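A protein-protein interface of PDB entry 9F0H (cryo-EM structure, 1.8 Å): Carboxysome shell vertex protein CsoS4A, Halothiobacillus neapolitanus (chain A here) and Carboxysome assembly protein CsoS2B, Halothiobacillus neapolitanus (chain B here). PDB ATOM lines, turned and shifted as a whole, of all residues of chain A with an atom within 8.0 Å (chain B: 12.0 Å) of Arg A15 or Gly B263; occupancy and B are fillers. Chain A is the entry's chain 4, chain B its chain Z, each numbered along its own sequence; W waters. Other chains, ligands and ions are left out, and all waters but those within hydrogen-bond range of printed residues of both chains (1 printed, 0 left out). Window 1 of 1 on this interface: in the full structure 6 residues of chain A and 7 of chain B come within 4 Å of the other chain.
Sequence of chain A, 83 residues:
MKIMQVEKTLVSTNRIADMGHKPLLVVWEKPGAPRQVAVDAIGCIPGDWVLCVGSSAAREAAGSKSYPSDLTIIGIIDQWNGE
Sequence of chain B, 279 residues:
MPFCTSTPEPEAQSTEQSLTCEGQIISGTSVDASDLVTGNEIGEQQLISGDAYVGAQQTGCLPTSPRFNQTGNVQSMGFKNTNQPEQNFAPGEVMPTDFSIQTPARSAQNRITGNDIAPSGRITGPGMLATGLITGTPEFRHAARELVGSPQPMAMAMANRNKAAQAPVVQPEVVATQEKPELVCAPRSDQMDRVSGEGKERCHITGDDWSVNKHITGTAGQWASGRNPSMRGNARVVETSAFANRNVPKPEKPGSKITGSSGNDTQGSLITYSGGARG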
ATOM      1  N   LEU A  10     -26.175  12.654  17.715  1.00  0.00           N
ATOM      2  CA  LEU A  10     -25.077  13.597  17.579  1.00  0.00           C
ATOM      3  C   LEU A  10     -25.638  14.918  17.086  1.00  0.00           C
ATOM      4  O   LEU A  10     -26.372  14.947  16.096  1.00  0.00           O
ATOM      5  CB  LEU A  10     -24.024  13.059  16.607  1.00  0.00           C
ATOM      6  CG  LEU A  10     -22.600  13.610  16.599  1.00  0.00           C
ATOM      7  CD1 LEU A  10     -22.543  14.938  15.883  1.00  0.00           C
ATOM      8  CD2 LEU A  10     -22.068  13.737  18.001  1.00  0.00           C
ATOM      9  N   VAL A  11     -25.296  16.005  17.766  1.00  0.00           N
ATOM     10  CA  VAL A  11     -25.805  17.327  17.428  1.00  0.00           C
ATOM     11  C   VAL A  11     -24.633  18.259  17.163  1.00  0.00           C
ATOM     12  O   VAL A  11     -23.734  18.390  17.998  1.00  0.00           O
ATOM     13  CB  VAL A  11     -26.707  17.888  18.540  1.00  0.00           C
ATOM     14  CG1 VAL A  11     -27.052  19.329  18.256  1.00  0.00           C
ATOM     15  CG2 VAL A  11     -27.961  17.057  18.651  1.00  0.00           C
ATOM     16  N   SER A  12     -24.653  18.906  16.005  1.00  0.00           N
ATOM     17  CA  SER A  12     -23.654  19.901  15.633  1.00  0.00           C
ATOM     18  C   SER A  12     -24.409  21.109  15.097  1.00  0.00           C
ATOM     19  O   SER A  12     -24.840  21.115  13.943  1.00  0.00           O
ATOM     20  CB  SER A  12     -22.680  19.351  14.605  1.00  0.00           C
ATOM     21  OG  SER A  12     -21.774  20.350  14.191  1.00  0.00           O
ATOM     22  N   THR A  13     -24.570  22.129  15.935  1.00  0.00           N
ATOM     23  CA  THR A  13     -25.388  23.270  15.550  1.00  0.00           C
ATOM     24  C   THR A  13     -24.766  24.046  14.396  1.00  0.00           C
ATOM     25  O   THR A  13     -25.478  24.502  13.497  1.00  0.00           O
ATOM     26  CB  THR A  13     -25.613  24.180  16.752  1.00  0.00           C
ATOM     27  OG1 THR A  13     -26.208  23.423  17.810  1.00  0.00           O
ATOM     28  CG2 THR A  13     -26.528  25.325  16.388  1.00  0.00           C
ATOM     29  N   ASN A  14     -23.446  24.199  14.392  1.00  0.00           N
ATOM     30  CA  ASN A  14     -22.779  25.020  13.394  1.00  0.00           C
ATOM     31  C   ASN A  14     -22.315  24.227  12.174  1.00  0.00           C
ATOM     32  O   ASN A  14     -21.434  24.691  11.449  1.00  0.00           O
ATOM     33  CB  ASN A  14     -21.600  25.753  14.026  1.00  0.00           C
ATOM     34  CG  ASN A  14     -20.388  24.884  14.168  1.00  0.00           C
ATOM     35  OD1 ASN A  14     -20.494  23.700  14.457  1.00  0.00           O
ATOM     36  ND2 ASN A  14     -19.221  25.469  13.970  1.00  0.00           N
ATOM     37  N   ARG A  15     -22.897  23.063  11.918  1.00  0.00           N
ATOM     38  CA  ARG A  15     -22.489  22.258  10.780  1.00  0.00           C
ATOM     39  C   ARG A  15     -22.779  22.985   9.469  1.00  0.00           C
ATOM     40  O   ARG A  15     -23.552  23.938   9.414  1.00  0.00           O
ATOM     41  CB  ARG A  15     -23.209  20.917  10.803  1.00  0.00           C
ATOM     42  CG  ARG A  15     -24.676  21.025  10.500  1.00  0.00           C
ATOM     43  CD  ARG A  15     -25.420  19.811  10.973  1.00  0.00           C
ATOM     44  NE  ARG A  15     -26.625  19.592  10.187  1.00  0.00           N
ATOM     45  CZ  ARG A  15     -27.415  18.540  10.320  1.00  0.00           C
ATOM     46  NH1 ARG A  15     -27.166  17.602  11.213  1.00  0.00           N
ATOM     47  NH2 ARG A  15     -28.482  18.428   9.538  1.00  0.00           N
ATOM     48  N   ILE A  16     -22.140  22.517   8.396  1.00  0.00           N
ATOM     49  CA  ILE A  16     -22.276  23.188   7.112  1.00  0.00           C
ATOM     50  C   ILE A  16     -23.718  23.108   6.627  1.00  0.00           C
ATOM     51  O   ILE A  16     -24.474  22.200   6.989  1.00  0.00           O
ATOM     52  CB  ILE A  16     -21.317  22.594   6.069  1.00  0.00           C
ATOM     53  CG1 ILE A  16     -21.583  21.105   5.892  1.00  0.00           C
ATOM     54  CG2 ILE A  16     -19.883  22.827   6.474  1.00  0.00           C
ATOM     55  CD1 ILE A  16     -20.862  20.498   4.736  1.00  0.00           C
ATOM     56  N   ALA A  17     -24.101  24.073   5.793  1.00  0.00           N
ATOM     57  CA  ALA A  17     -25.484  24.162   5.345  1.00  0.00           C
ATOM     58  C   ALA A  17     -25.862  23.020   4.415  1.00  0.00           C
ATOM     59  O   ALA A  17     -27.041  22.671   4.319  1.00  0.00           O
ATOM     60  CB  ALA A  17     -25.726  25.500   4.654  1.00  0.00           C
ATOM     61  N   ASP A  18     -24.891  22.433   3.720  1.00  0.00           N
ATOM     62  CA  ASP A  18     -25.188  21.370   2.772  1.00  0.00           C
ATOM     63  C   ASP A  18     -25.635  20.081   3.442  1.00  0.00           C
ATOM     64  O   ASP A  18     -26.143  19.195   2.752  1.00  0.00           O
ATOM     65  CB  ASP A  18     -23.973  21.109   1.893  1.00  0.00           C
ATOM     66  CG  ASP A  18     -23.793  22.171   0.827  1.00  0.00           C
ATOM     67  OD1 ASP A  18     -24.667  23.052   0.710  1.00  0.00           O
ATOM     68  OD2 ASP A  18     -22.774  22.132   0.110  1.00  0.00           O
ATOM     69  N   MET A  19     -25.476  19.956   4.755  1.00  0.00           N
ATOM     70  CA  MET A  19     -25.999  18.797   5.459  1.00  0.00           C
ATOM     71  C   MET A  19     -27.518  18.792   5.540  1.00  0.00           C
ATOM     72  O   MET A  19     -28.092  17.776   5.936  1.00  0.00           O
ATOM     73  CB  MET A  19     -25.410  18.735   6.861  1.00  0.00           C
ATOM     74  CG  MET A  19     -23.933  18.453   6.875  1.00  0.00           C
ATOM     75  SD  MET A  19     -23.420  17.550   8.329  1.00  0.00           S
ATOM     76  CE  MET A  19     -23.529  15.882   7.698  1.00  0.00           C
ATOM     77  N   GLY A  20     -28.177  19.889   5.181  1.00  0.00           N
ATOM     78  CA  GLY A  20     -29.622  19.913   5.223  1.00  0.00           C
ATOM     79  C   GLY A  20     -30.146  19.791   6.642  1.00  0.00           C
ATOM     80  O   GLY A  20     -29.552  20.284   7.600  1.00  0.00           O
ATOM     81  N   HIS A  21     -31.281  19.114   6.775  1.00  0.00           N
ATOM     82  CA  HIS A  21     -31.903  18.888   8.069  1.00  0.00           C
ATOM     83  C   HIS A  21     -31.717  17.469   8.582  1.00  0.00           C
ATOM     84  O   HIS A  21     -32.374  17.087   9.550  1.00  0.00           O
ATOM     85  CB  HIS A  21     -33.392  19.215   8.002  1.00  0.00           C
ATOM     86  CG  HIS A  21     -33.686  20.657   7.751  1.00  0.00           C
ATOM     87  ND1 HIS A  21     -34.906  21.095   7.292  1.00  0.00           N
ATOM     88  CD2 HIS A  21     -32.924  21.764   7.912  1.00  0.00           C
ATOM     89  CE1 HIS A  21     -34.883  22.409   7.173  1.00  0.00           C
ATOM     90  NE2 HIS A  21     -33.693  22.839   7.541  1.00  0.00           N
ATOM     91  N   LYS A  22     -30.849  16.682   7.963  1.00  0.00           N
ATOM     92  CA  LYS A  22     -30.753  15.271   8.305  1.00  0.00           C
ATOM     93  C   LYS A  22     -30.218  15.087   9.722  1.00  0.00           C
ATOM     94  O   LYS A  22     -29.332  15.822  10.151  1.00  0.00           O
ATOM     95  CB  LYS A  22     -29.846  14.548   7.320  1.00  0.00           C
ATOM     96  CG  LYS A  22     -30.275  14.683   5.883  1.00  0.00           C
ATOM     97  CD  LYS A  22     -31.320  13.656   5.529  1.00  0.00           C
ATOM     98  CE  LYS A  22     -32.010  14.005   4.225  1.00  0.00           C
ATOM     99  NZ  LYS A  22     -31.281  15.065   3.483  1.00  0.00           N
ATOM    100  N   PRO A  23     -30.731  14.116  10.468  1.00  0.00           N
ATOM    101  CA  PRO A  23     -30.177  13.817  11.786  1.00  0.00           C
ATOM    102  C   PRO A  23     -28.944  12.934  11.689  1.00  0.00           C
ATOM    103  O   PRO A  23     -28.731  12.224  10.710  1.00  0.00           O
ATOM    104  CB  PRO A  23     -31.320  13.079  12.484  1.00  0.00           C
ATOM    105  CG  PRO A  23     -32.048  12.428  11.389  1.00  0.00           C
ATOM    106  CD  PRO A  23     -31.900  13.278  10.161  1.00  0.00           C
ATOM    107  N   LEU A  24     -28.136  12.978  12.740  1.00  0.00           N
ATOM    108  CA  LEU A  24     -26.900  12.220  12.820  1.00  0.00           C
ATOM    109  C   LEU A  24     -26.925  11.315  14.039  1.00  0.00           C
ATOM    110  O   LEU A  24     -27.474  11.673  15.080  1.00  0.00           O
ATOM    111  CB  LEU A  24     -25.688  13.141  12.904  1.00  0.00           C
ATOM    112  CG  LEU A  24     -25.617  14.262  11.877  1.00  0.00           C
ATOM    113  CD1 LEU A  24     -24.456  15.166  12.186  1.00  0.00           C
ATOM    114  CD2 LEU A  24     -25.494  13.702  10.479  1.00  0.00           C
ATOM    115  N   LEU A  25     -26.313  10.146  13.908  1.00  0.00           N
ATOM    116  CA  LEU A  25     -26.283   9.162  14.978  1.00  0.00           C
ATOM    117  C   LEU A  25     -24.865   8.666  15.189  1.00  0.00           C
ATOM    118  O   LEU A  25     -24.084   8.556  14.246  1.00  0.00           O
ATOM    119  CB  LEU A  25     -27.190   7.975  14.671  1.00  0.00           C
ATOM    120  CG  LEU A  25     -28.680   8.266  14.558  1.00  0.00           C
ATOM    121  CD1 LEU A  25     -29.410   6.997  14.230  1.00  0.00           C
ATOM    122  CD2 LEU A  25     -29.199   8.854  15.845  1.00  0.00           C
ATOM    123  N   VAL A  39     -25.324   9.477   8.822  1.00  0.00           N
ATOM    124  CA  VAL A  39     -26.595  10.114   8.522  1.00  0.00           C
ATOM    125  C   VAL A  39     -27.697   9.075   8.652  1.00  0.00           C
ATOM    126  O   VAL A  39     -27.598   7.974   8.102  1.00  0.00           O
ATOM    127  CB  VAL A  39     -26.572  10.724   7.115  1.00  0.00           C
ATOM    128  CG1 VAL A  39     -27.964  11.130   6.697  1.00  0.00           C
ATOM    129  CG2 VAL A  39     -25.639  11.902   7.065  1.00  0.00           C
ATOM    130  N   TYR A  67     -24.599  15.249  -1.706  1.00  0.00           N
ATOM    131  CA  TYR A  67     -24.763  15.365  -0.268  1.00  0.00           C
ATOM    132  C   TYR A  67     -23.448  15.056   0.444  1.00  0.00           C
ATOM    133  O   TYR A  67     -22.757  14.102   0.085  1.00  0.00           O
ATOM    134  CB  TYR A  67     -25.849  14.425   0.234  1.00  0.00           C
ATOM    135  CG  TYR A  67     -26.192  14.682   1.672  1.00  0.00           C
ATOM    136  CD1 TYR A  67     -25.486  14.073   2.691  1.00  0.00           C
ATOM    137  CD2 TYR A  67     -27.199  15.561   2.011  1.00  0.00           C
ATOM    138  CE1 TYR A  67     -25.780  14.322   4.000  1.00  0.00           C
ATOM    139  CE2 TYR A  67     -27.501  15.813   3.319  1.00  0.00           C
ATOM    140  CZ  TYR A  67     -26.787  15.192   4.310  1.00  0.00           C
ATOM    141  OH  TYR A  67     -27.081  15.435   5.625  1.00  0.00           O
ATOM    142  N   GLY B 255     -36.793  35.186   4.853  1.00  0.00           N
ATOM    143  CA  GLY B 255     -35.470  34.837   4.394  1.00  0.00           C
ATOM    144  C   GLY B 255     -34.479  34.825   5.542  1.00  0.00           C
ATOM    145  O   GLY B 255     -34.795  35.159   6.676  1.00  0.00           O
ATOM    146  N   SER B 256     -33.256  34.417   5.227  1.00  0.00           N
ATOM    147  CA  SER B 256     -32.182  34.384   6.207  1.00  0.00           C
ATOM    148  C   SER B 256     -30.972  35.104   5.636  1.00  0.00           C
ATOM    149  O   SER B 256     -30.542  34.805   4.519  1.00  0.00           O
ATOM    150  CB  SER B 256     -31.825  32.948   6.584  1.00  0.00           C
ATOM    151  OG  SER B 256     -30.803  32.923   7.557  1.00  0.00           O
ATOM    152  N   LYS B 257     -30.428  36.047   6.398  1.00  0.00           N
ATOM    153  CA  LYS B 257     -29.285  36.835   5.960  1.00  0.00           C
ATOM    154  C   LYS B 257     -28.044  36.595   6.805  1.00  0.00           C
ATOM    155  O   LYS B 257     -27.041  37.285   6.620  1.00  0.00           O
ATOM    156  CB  LYS B 257     -29.634  38.321   5.972  1.00  0.00           C
ATOM    157  CG  LYS B 257     -30.383  38.789   4.749  1.00  0.00           C
ATOM    158  CD  LYS B 257     -31.307  39.935   5.091  1.00  0.00           C
ATOM    159  CE  LYS B 257     -31.986  40.478   3.853  1.00  0.00           C
ATOM    160  NZ  LYS B 257     -31.034  40.595   2.723  1.00  0.00           N
ATOM    161  N   ILE B 258     -28.081  35.638   7.726  1.00  0.00           N
ATOM    162  CA  ILE B 258     -26.969  35.455   8.642  1.00  0.00           C
ATOM    163  C   ILE B 258     -25.822  34.741   7.940  1.00  0.00           C
ATOM    164  O   ILE B 258     -26.024  33.945   7.018  1.00  0.00           O
ATOM    165  CB  ILE B 258     -27.439  34.685   9.887  1.00  0.00           C
ATOM    166  CG1 ILE B 258     -27.937  33.305   9.499  1.00  0.00           C
ATOM    167  CG2 ILE B 258     -28.566  35.426  10.561  1.00  0.00           C
ATOM    168  CD1 ILE B 258     -27.567  32.255  10.477  1.00  0.00           C
ATOM    169  N   THR B 259     -24.602  35.047   8.361  1.00  0.00           N
ATOM    170  CA  THR B 259     -23.407  34.400   7.848  1.00  0.00           C
ATOM    171  C   THR B 259     -22.723  33.635   8.970  1.00  0.00           C
ATOM    172  O   THR B 259     -23.100  33.722  10.137  1.00  0.00           O
ATOM    173  CB  THR B 259     -22.431  35.407   7.224  1.00  0.00           C
ATOM    174  OG1 THR B 259     -22.122  36.436   8.167  1.00  0.00           O
ATOM    175  CG2 THR B 259     -23.024  36.029   5.977  1.00  0.00           C
ATOM    176  N   GLY B 260     -21.706  32.883   8.601  1.00  0.00           N
ATOM    177  CA  GLY B 260     -21.101  31.959   9.541  1.00  0.00           C
ATOM    178  C   GLY B 260     -21.805  30.619   9.532  1.00  0.00           C
ATOM    179  O   GLY B 260     -23.008  30.517   9.306  1.00  0.00           O
ATOM    180  N   SER B 261     -21.036  29.569   9.784  1.00  0.00           N
ATOM    181  CA  SER B 261     -21.578  28.218   9.696  1.00  0.00           C
ATOM    182  C   SER B 261     -22.601  27.996  10.801  1.00  0.00           C
ATOM    183  O   SER B 261     -22.261  28.016  11.986  1.00  0.00           O
ATOM    184  CB  SER B 261     -20.456  27.194   9.784  1.00  0.00           C
ATOM    185  OG  SER B 261     -19.764  27.324  11.006  1.00  0.00           O
ATOM    186  N   SER B 262     -23.864  27.823  10.412  1.00  0.00           N
ATOM    187  CA  SER B 262     -24.933  27.648  11.386  1.00  0.00           C
ATOM    188  C   SER B 262     -25.982  26.655  10.910  1.00  0.00           C
ATOM    189  O   SER B 262     -27.133  26.719  11.353  1.00  0.00           O
ATOM    190  CB  SER B 262     -25.591  28.986  11.692  1.00  0.00           C
ATOM    191  OG  SER B 262     -25.816  29.706  10.498  1.00  0.00           O
ATOM    192  N   GLY B 263     -25.619  25.753  10.007  1.00  0.00           N
ATOM    193  CA  GLY B 263     -26.600  24.861   9.413  1.00  0.00           C
ATOM    194  C   GLY B 263     -27.679  25.592   8.649  1.00  0.00           C
ATOM    195  O   GLY B 263     -28.849  25.200   8.703  1.00  0.00           O
ATOM    196  N   ASN B 264     -27.310  26.647   7.924  1.00  0.00           N
ATOM    197  CA  ASN B 264     -28.280  27.559   7.319  1.00  0.00           C
ATOM    198  C   ASN B 264     -28.776  27.005   5.984  1.00  0.00           C
ATOM    199  O   ASN B 264     -28.543  27.559   4.908  1.00  0.00           O
ATOM    200  CB  ASN B 264     -27.668  28.939   7.148  1.00  0.00           C
ATOM    201  CG  ASN B 264     -28.709  30.021   7.004  1.00  0.00           C
ATOM    202  OD1 ASN B 264     -29.799  29.925   7.559  1.00  0.00           O
ATOM    203  ND2 ASN B 264     -28.380  31.060   6.253  1.00  0.00           N
ATOM    204  N   ASP B 265     -29.496  25.894   6.070  1.00  0.00           N
ATOM    205  CA  ASP B 265     -30.102  25.314   4.880  1.00  0.00           C
ATOM    206  C   ASP B 265     -31.291  26.154   4.433  1.00  0.00           C
ATOM    207  O   ASP B 265     -32.059  26.658   5.254  1.00  0.00           O
ATOM    208  CB  ASP B 265     -30.546  23.881   5.155  1.00  0.00           C
ATOM    209  CG  ASP B 265     -31.472  23.345   4.085  1.00  0.00           C
ATOM    210  OD1 ASP B 265     -30.973  22.940   3.018  1.00  0.00           O
ATOM    211  OD2 ASP B 265     -32.698  23.332   4.305  1.00  0.00           O
ATOM    212  N   THR B 266     -31.436  26.311   3.122  1.00  0.00           N
ATOM    213  CA  THR B 266     -32.561  27.036   2.554  1.00  0.00           C
ATOM    214  C   THR B 266     -33.427  26.180   1.646  1.00  0.00           C
ATOM    215  O   THR B 266     -34.408  26.688   1.095  1.00  0.00           O
ATOM    216  CB  THR B 266     -32.072  28.262   1.773  1.00  0.00           C
ATOM    217  OG1 THR B 266     -31.393  27.834   0.588  1.00  0.00           O
ATOM    218  CG2 THR B 266     -31.129  29.095   2.617  1.00  0.00           C
ATOM    219  N   GLN B 267     -33.104  24.902   1.479  1.00  0.00           N
ATOM    220  CA  GLN B 267     -33.834  24.040   0.563  1.00  0.00           C
ATOM    221  C   GLN B 267     -34.912  23.209   1.240  1.00  0.00           C
ATOM    222  O   GLN B 267     -35.863  22.799   0.569  1.00  0.00           O
ATOM    223  CB  GLN B 267     -32.867  23.097  -0.157  1.00  0.00           C
ATOM    224  CG  GLN B 267     -32.362  23.603  -1.493  1.00  0.00           C
ATOM    225  CD  GLN B 267     -32.152  25.100  -1.512  1.00  0.00           C
ATOM    226  OE1 GLN B 267     -31.110  25.594  -1.086  1.00  0.00           O
ATOM    227  NE2 GLN B 267     -33.134  25.833  -2.025  1.00  0.00           N
ATOM    228  N   GLY B 268     -34.797  22.962   2.535  1.00  0.00           N
ATOM    229  CA  GLY B 268     -35.693  22.057   3.217  1.00  0.00           C
ATOM    230  C   GLY B 268     -36.994  22.713   3.624  1.00  0.00           C
ATOM    231  O   GLY B 268     -37.424  23.723   3.064  1.00  0.00           O
ATOM    232  N   SER B 269     -37.634  22.110   4.619  1.00  0.00           N
ATOM    233  CA  SER B 269     -38.884  22.633   5.135  1.00  0.00           C
ATOM    234  C   SER B 269     -38.658  23.975   5.821  1.00  0.00           C
ATOM    235  O   SER B 269     -37.555  24.303   6.261  1.00  0.00           O
ATOM    236  CB  SER B 269     -39.513  21.647   6.115  1.00  0.00           C
ATOM    237  OG  SER B 269     -39.989  20.502   5.438  1.00  0.00           O
ATOM    238  N   LEU B 270     -39.724  24.757   5.900  1.00  0.00           N
ATOM    239  CA  LEU B 270     -39.658  26.056   6.547  1.00  0.00           C
ATOM    240  C   LEU B 270     -39.715  25.878   8.058  1.00  0.00           C
ATOM    241  O   LEU B 270     -40.719  25.409   8.597  1.00  0.00           O
ATOM    242  CB  LEU B 270     -40.798  26.948   6.065  1.00  0.00           C
ATOM    243  CG  LEU B 270     -41.069  28.186   6.914  1.00  0.00           C
ATOM    244  CD1 LEU B 270     -39.871  29.107   6.906  1.00  0.00           C
ATOM    245  CD2 LEU B 270     -42.302  28.913   6.421  1.00  0.00           C
ATOM    246  N   ILE B 271     -38.639  26.258   8.734  1.00  0.00           N
ATOM    247  CA  ILE B 271     -38.580  26.319  10.186  1.00  0.00           C
ATOM    248  C   ILE B 271     -38.609  27.781  10.588  1.00  0.00           C
ATOM    249  O   ILE B 271     -37.962  28.616   9.951  1.00  0.00           O
ATOM    250  CB  ILE B 271     -37.311  25.646  10.739  1.00  0.00           C
ATOM    251  CG1 ILE B 271     -36.962  24.411   9.919  1.00  0.00           C
ATOM    252  CG2 ILE B 271     -37.488  25.317  12.198  1.00  0.00           C
ATOM    253  CD1 ILE B 271     -37.875  23.280  10.157  1.00  0.00           C
ATOM    254  N   THR B 272     -39.356  28.096  11.634  1.00  0.00           N
ATOM    255  CA  THR B 272     -39.425  29.457  12.131  1.00  0.00           C
ATOM    256  C   THR B 272     -38.933  29.518  13.566  1.00  0.00           C
ATOM    257  O   THR B 272     -39.065  28.561  14.329  1.00  0.00           O
ATOM    258  CB  THR B 272     -40.848  30.029  12.046  1.00  0.00           C
ATOM    259  OG1 THR B 272     -41.801  29.031  12.423  1.00  0.00           O
ATOM    260  CG2 THR B 272     -41.146  30.500  10.636  1.00  0.00           C
ATOM    261  N   TYR B 273     -38.354  30.655  13.916  1.00  0.00           N
ATOM    262  CA  TYR B 273     -37.920  30.971  15.263  1.00  0.00           C
ATOM    263  C   TYR B 273     -38.804  32.071  15.832  1.00  0.00           C
ATOM    264  O   TYR B 273     -39.745  32.533  15.189  1.00  0.00           O
ATOM    265  CB  TYR B 273     -36.455  31.395  15.268  1.00  0.00           C
ATOM    266  CG  TYR B 273     -35.504  30.281  15.585  1.00  0.00           C
ATOM    267  CD1 TYR B 273     -35.147  30.002  16.889  1.00  0.00           C
ATOM    268  CD2 TYR B 273     -34.963  29.505  14.578  1.00  0.00           C
ATOM    269  CE1 TYR B 273     -34.276  28.986  17.180  1.00  0.00           C
ATOM    270  CE2 TYR B 273     -34.095  28.486  14.860  1.00  0.00           C
ATOM    271  CZ  TYR B 273     -33.753  28.230  16.161  1.00  0.00           C
ATOM    272  OH  TYR B 273     -32.886  27.213  16.451  1.00  0.00           O
ATOM    273  N   ALA B 277     -38.794  34.494  12.553  1.00  0.00           N
ATOM    274  CA  ALA B 277     -37.524  34.469  11.844  1.00  0.00           C
ATOM    275  C   ALA B 277     -37.249  33.088  11.264  1.00  0.00           C
ATOM    276  O   ALA B 277     -37.664  32.066  11.808  1.00  0.00           O
ATOM    277  CB  ALA B 277     -36.385  34.870  12.775  1.00  0.00           C
ATOM    278  N   ARG B 278     -36.527  33.069  10.150  1.00  0.00           N
ATOM    279  CA  ARG B 278     -36.227  31.820   9.466  1.00  0.00           C
ATOM    280  C   ARG B 278     -35.207  31.005  10.245  1.00  0.00           C
ATOM    281  O   ARG B 278     -34.159  31.518  10.641  1.00  0.00           O
ATOM    282  CB  ARG B 278     -35.701  32.107   8.068  1.00  0.00           C
ATOM    283  CG  ARG B 278     -35.346  30.872   7.290  1.00  0.00           C
ATOM    284  CD  ARG B 278     -36.544  30.383   6.536  1.00  0.00           C
ATOM    285  NE  ARG B 278     -36.275  29.158   5.798  1.00  0.00           N
ATOM    286  CZ  ARG B 278     -36.283  29.073   4.478  1.00  0.00           C
ATOM    287  NH1 ARG B 278     -36.515  30.131   3.721  1.00  0.00           N
ATOM    288  NH2 ARG B 278     -36.057  27.898   3.904  1.00  0.00           N
ATOM    289  N   GLY B 279     -35.505  29.729  10.445  1.00  0.00           N
ATOM    290  CA  GLY B 279     -34.618  28.838  11.165  1.00  0.00           C
ATOM    291  C   GLY B 279     -33.998  27.774  10.283  1.00  0.00           C
ATOM    292  O   GLY B 279     -33.290  26.886  10.756  1.00  0.00           O
ATOM    293  OXT GLY B 279     -34.190  27.763   9.070  1.00  0.00           O
HETATM  294  O   HOH W   1     -33.129  25.729   7.781  1.00  0.00           O
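A ring nitrogen (NE2) of His A21 is in hydrogen-bond range of the side-chain carboxylate (OD2) of Asp B265, 3.4 Å away. The backbone carbonyl oxygen of Asn A14 sits at hydrogen-bond distance from the side-chain hydroxyl of Ser B261, at 3.1 Å. N of Gly B263 lies within hydrogen-bond range of O of Arg A15, at 2.8 Å.
The guanidinium group of Arg A15 is in hydrogen-bond range of the backbone carbonyl oxygen of Lys A22, at 2.8 Å. OG of Ser B256 sits at hydrogen-bond distance from OD1 of Asn B264 (3.2 Å). O of Gly B260 is in hydrogen-bond range of OG of Ser B262 (3.2 Å). The backbone NH of Gly B279 lies within hydrogen-bond range of the backbone carbonyl oxygen of Ile B271 (2.7 Å). The backbone NH (N) of Gly B268 is in hydrogen-bond range of the side-chain carboxylate (OD2) of Asp B265 (2.8 Å). The guanidinium group (NH2) of Arg A15 sits at hydrogen-bond distance from the backbone carbonyl oxygen (O) of Gly A20 (2.9 Å).
O of Thr A13 touches C of Ser B262 (3.4 Å). Thr A13 touches Gly B263 (O to N, 3.7 Å). CA of Ser B262 touches CA of Asn A14, 3.9 Å away. O of Arg A15 touches C of Ser B262 (3.9 Å). Asn B264 touches Ala A17. Ala A17 touches Asp B265. Gly A20 touches Asp B265 (CA to OD1, 3.98 Å). His A21 touches Ser B269. His A21 touches Ile B271 (CE1 to CG1, 3.98 Å).
No residue of chain B comes within 4 Å of Val A11. No residue of chain B comes within 4 Å of Ser A12. Of chain B, only Ser B262 and Gly B263 come within 4 Å of Thr A13. Arg A15 touches just these residues of chain B: Ser B262 and Gly B263. No residue of chain B comes within 4 Å of Ile A16. Of the printed residues of chain B, Gly A20 touches Asp B265. No residue of chain B comes within 4 Å of Lys A22. No residue of chain B comes within 4 Å of Pro A23. No residue of chain B comes within 4 Å of Leu A24. Ile B258 touches none of the printed residues of chain A. Printed residues of chain A within 4 Å of Ser B261: Asn A14. Of the printed residues of chain A, Ser B262 touches Thr A13, Asn A14 and Arg A15. Of chain A, only Thr A13 and Arg A15 come within 4 Å of Gly B263. Printed residues of chain A within 4 Å of Asp B265: Ala A17, Gly A20 and His A21. Of the printed residues of chain A, Ser B269 touches His A21. The nearest residue of chain B that does not touch Arg A15 is Ser B261 (4.4 Å). The nearest residue of chain A that does not touch Gly B263 is Ile A16 (4.2 Å). The nearest printed residue of chain B that does not touch His A21 is Gly B268 (4.1 Å).
Hydrophobic or aromatic side chains of chain A that line the printed part of chain B: Ala A17 and His A21. Printed residues of chain B that touch a printed residue of chain A: Ser B261, Ser B262, Gly B263, Asn B264, Asp B265, Ser B269 and Ile B271. Hydrophobic or aromatic side chains of chain B that line the printed part of chain A: Ile B271. Among the printed residues, no Asp or Glu carboxylate lies within 4 Å of a Lys or Arg side-chain nitrogen of the other chain.
Water W1 lies within hydrogen-bond range of the chain-end carboxylate (OXT) of Gly B279, the backbone carbonyl oxygen (O) of Asp B265 and a ring nitrogen (NE2) of His A21.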
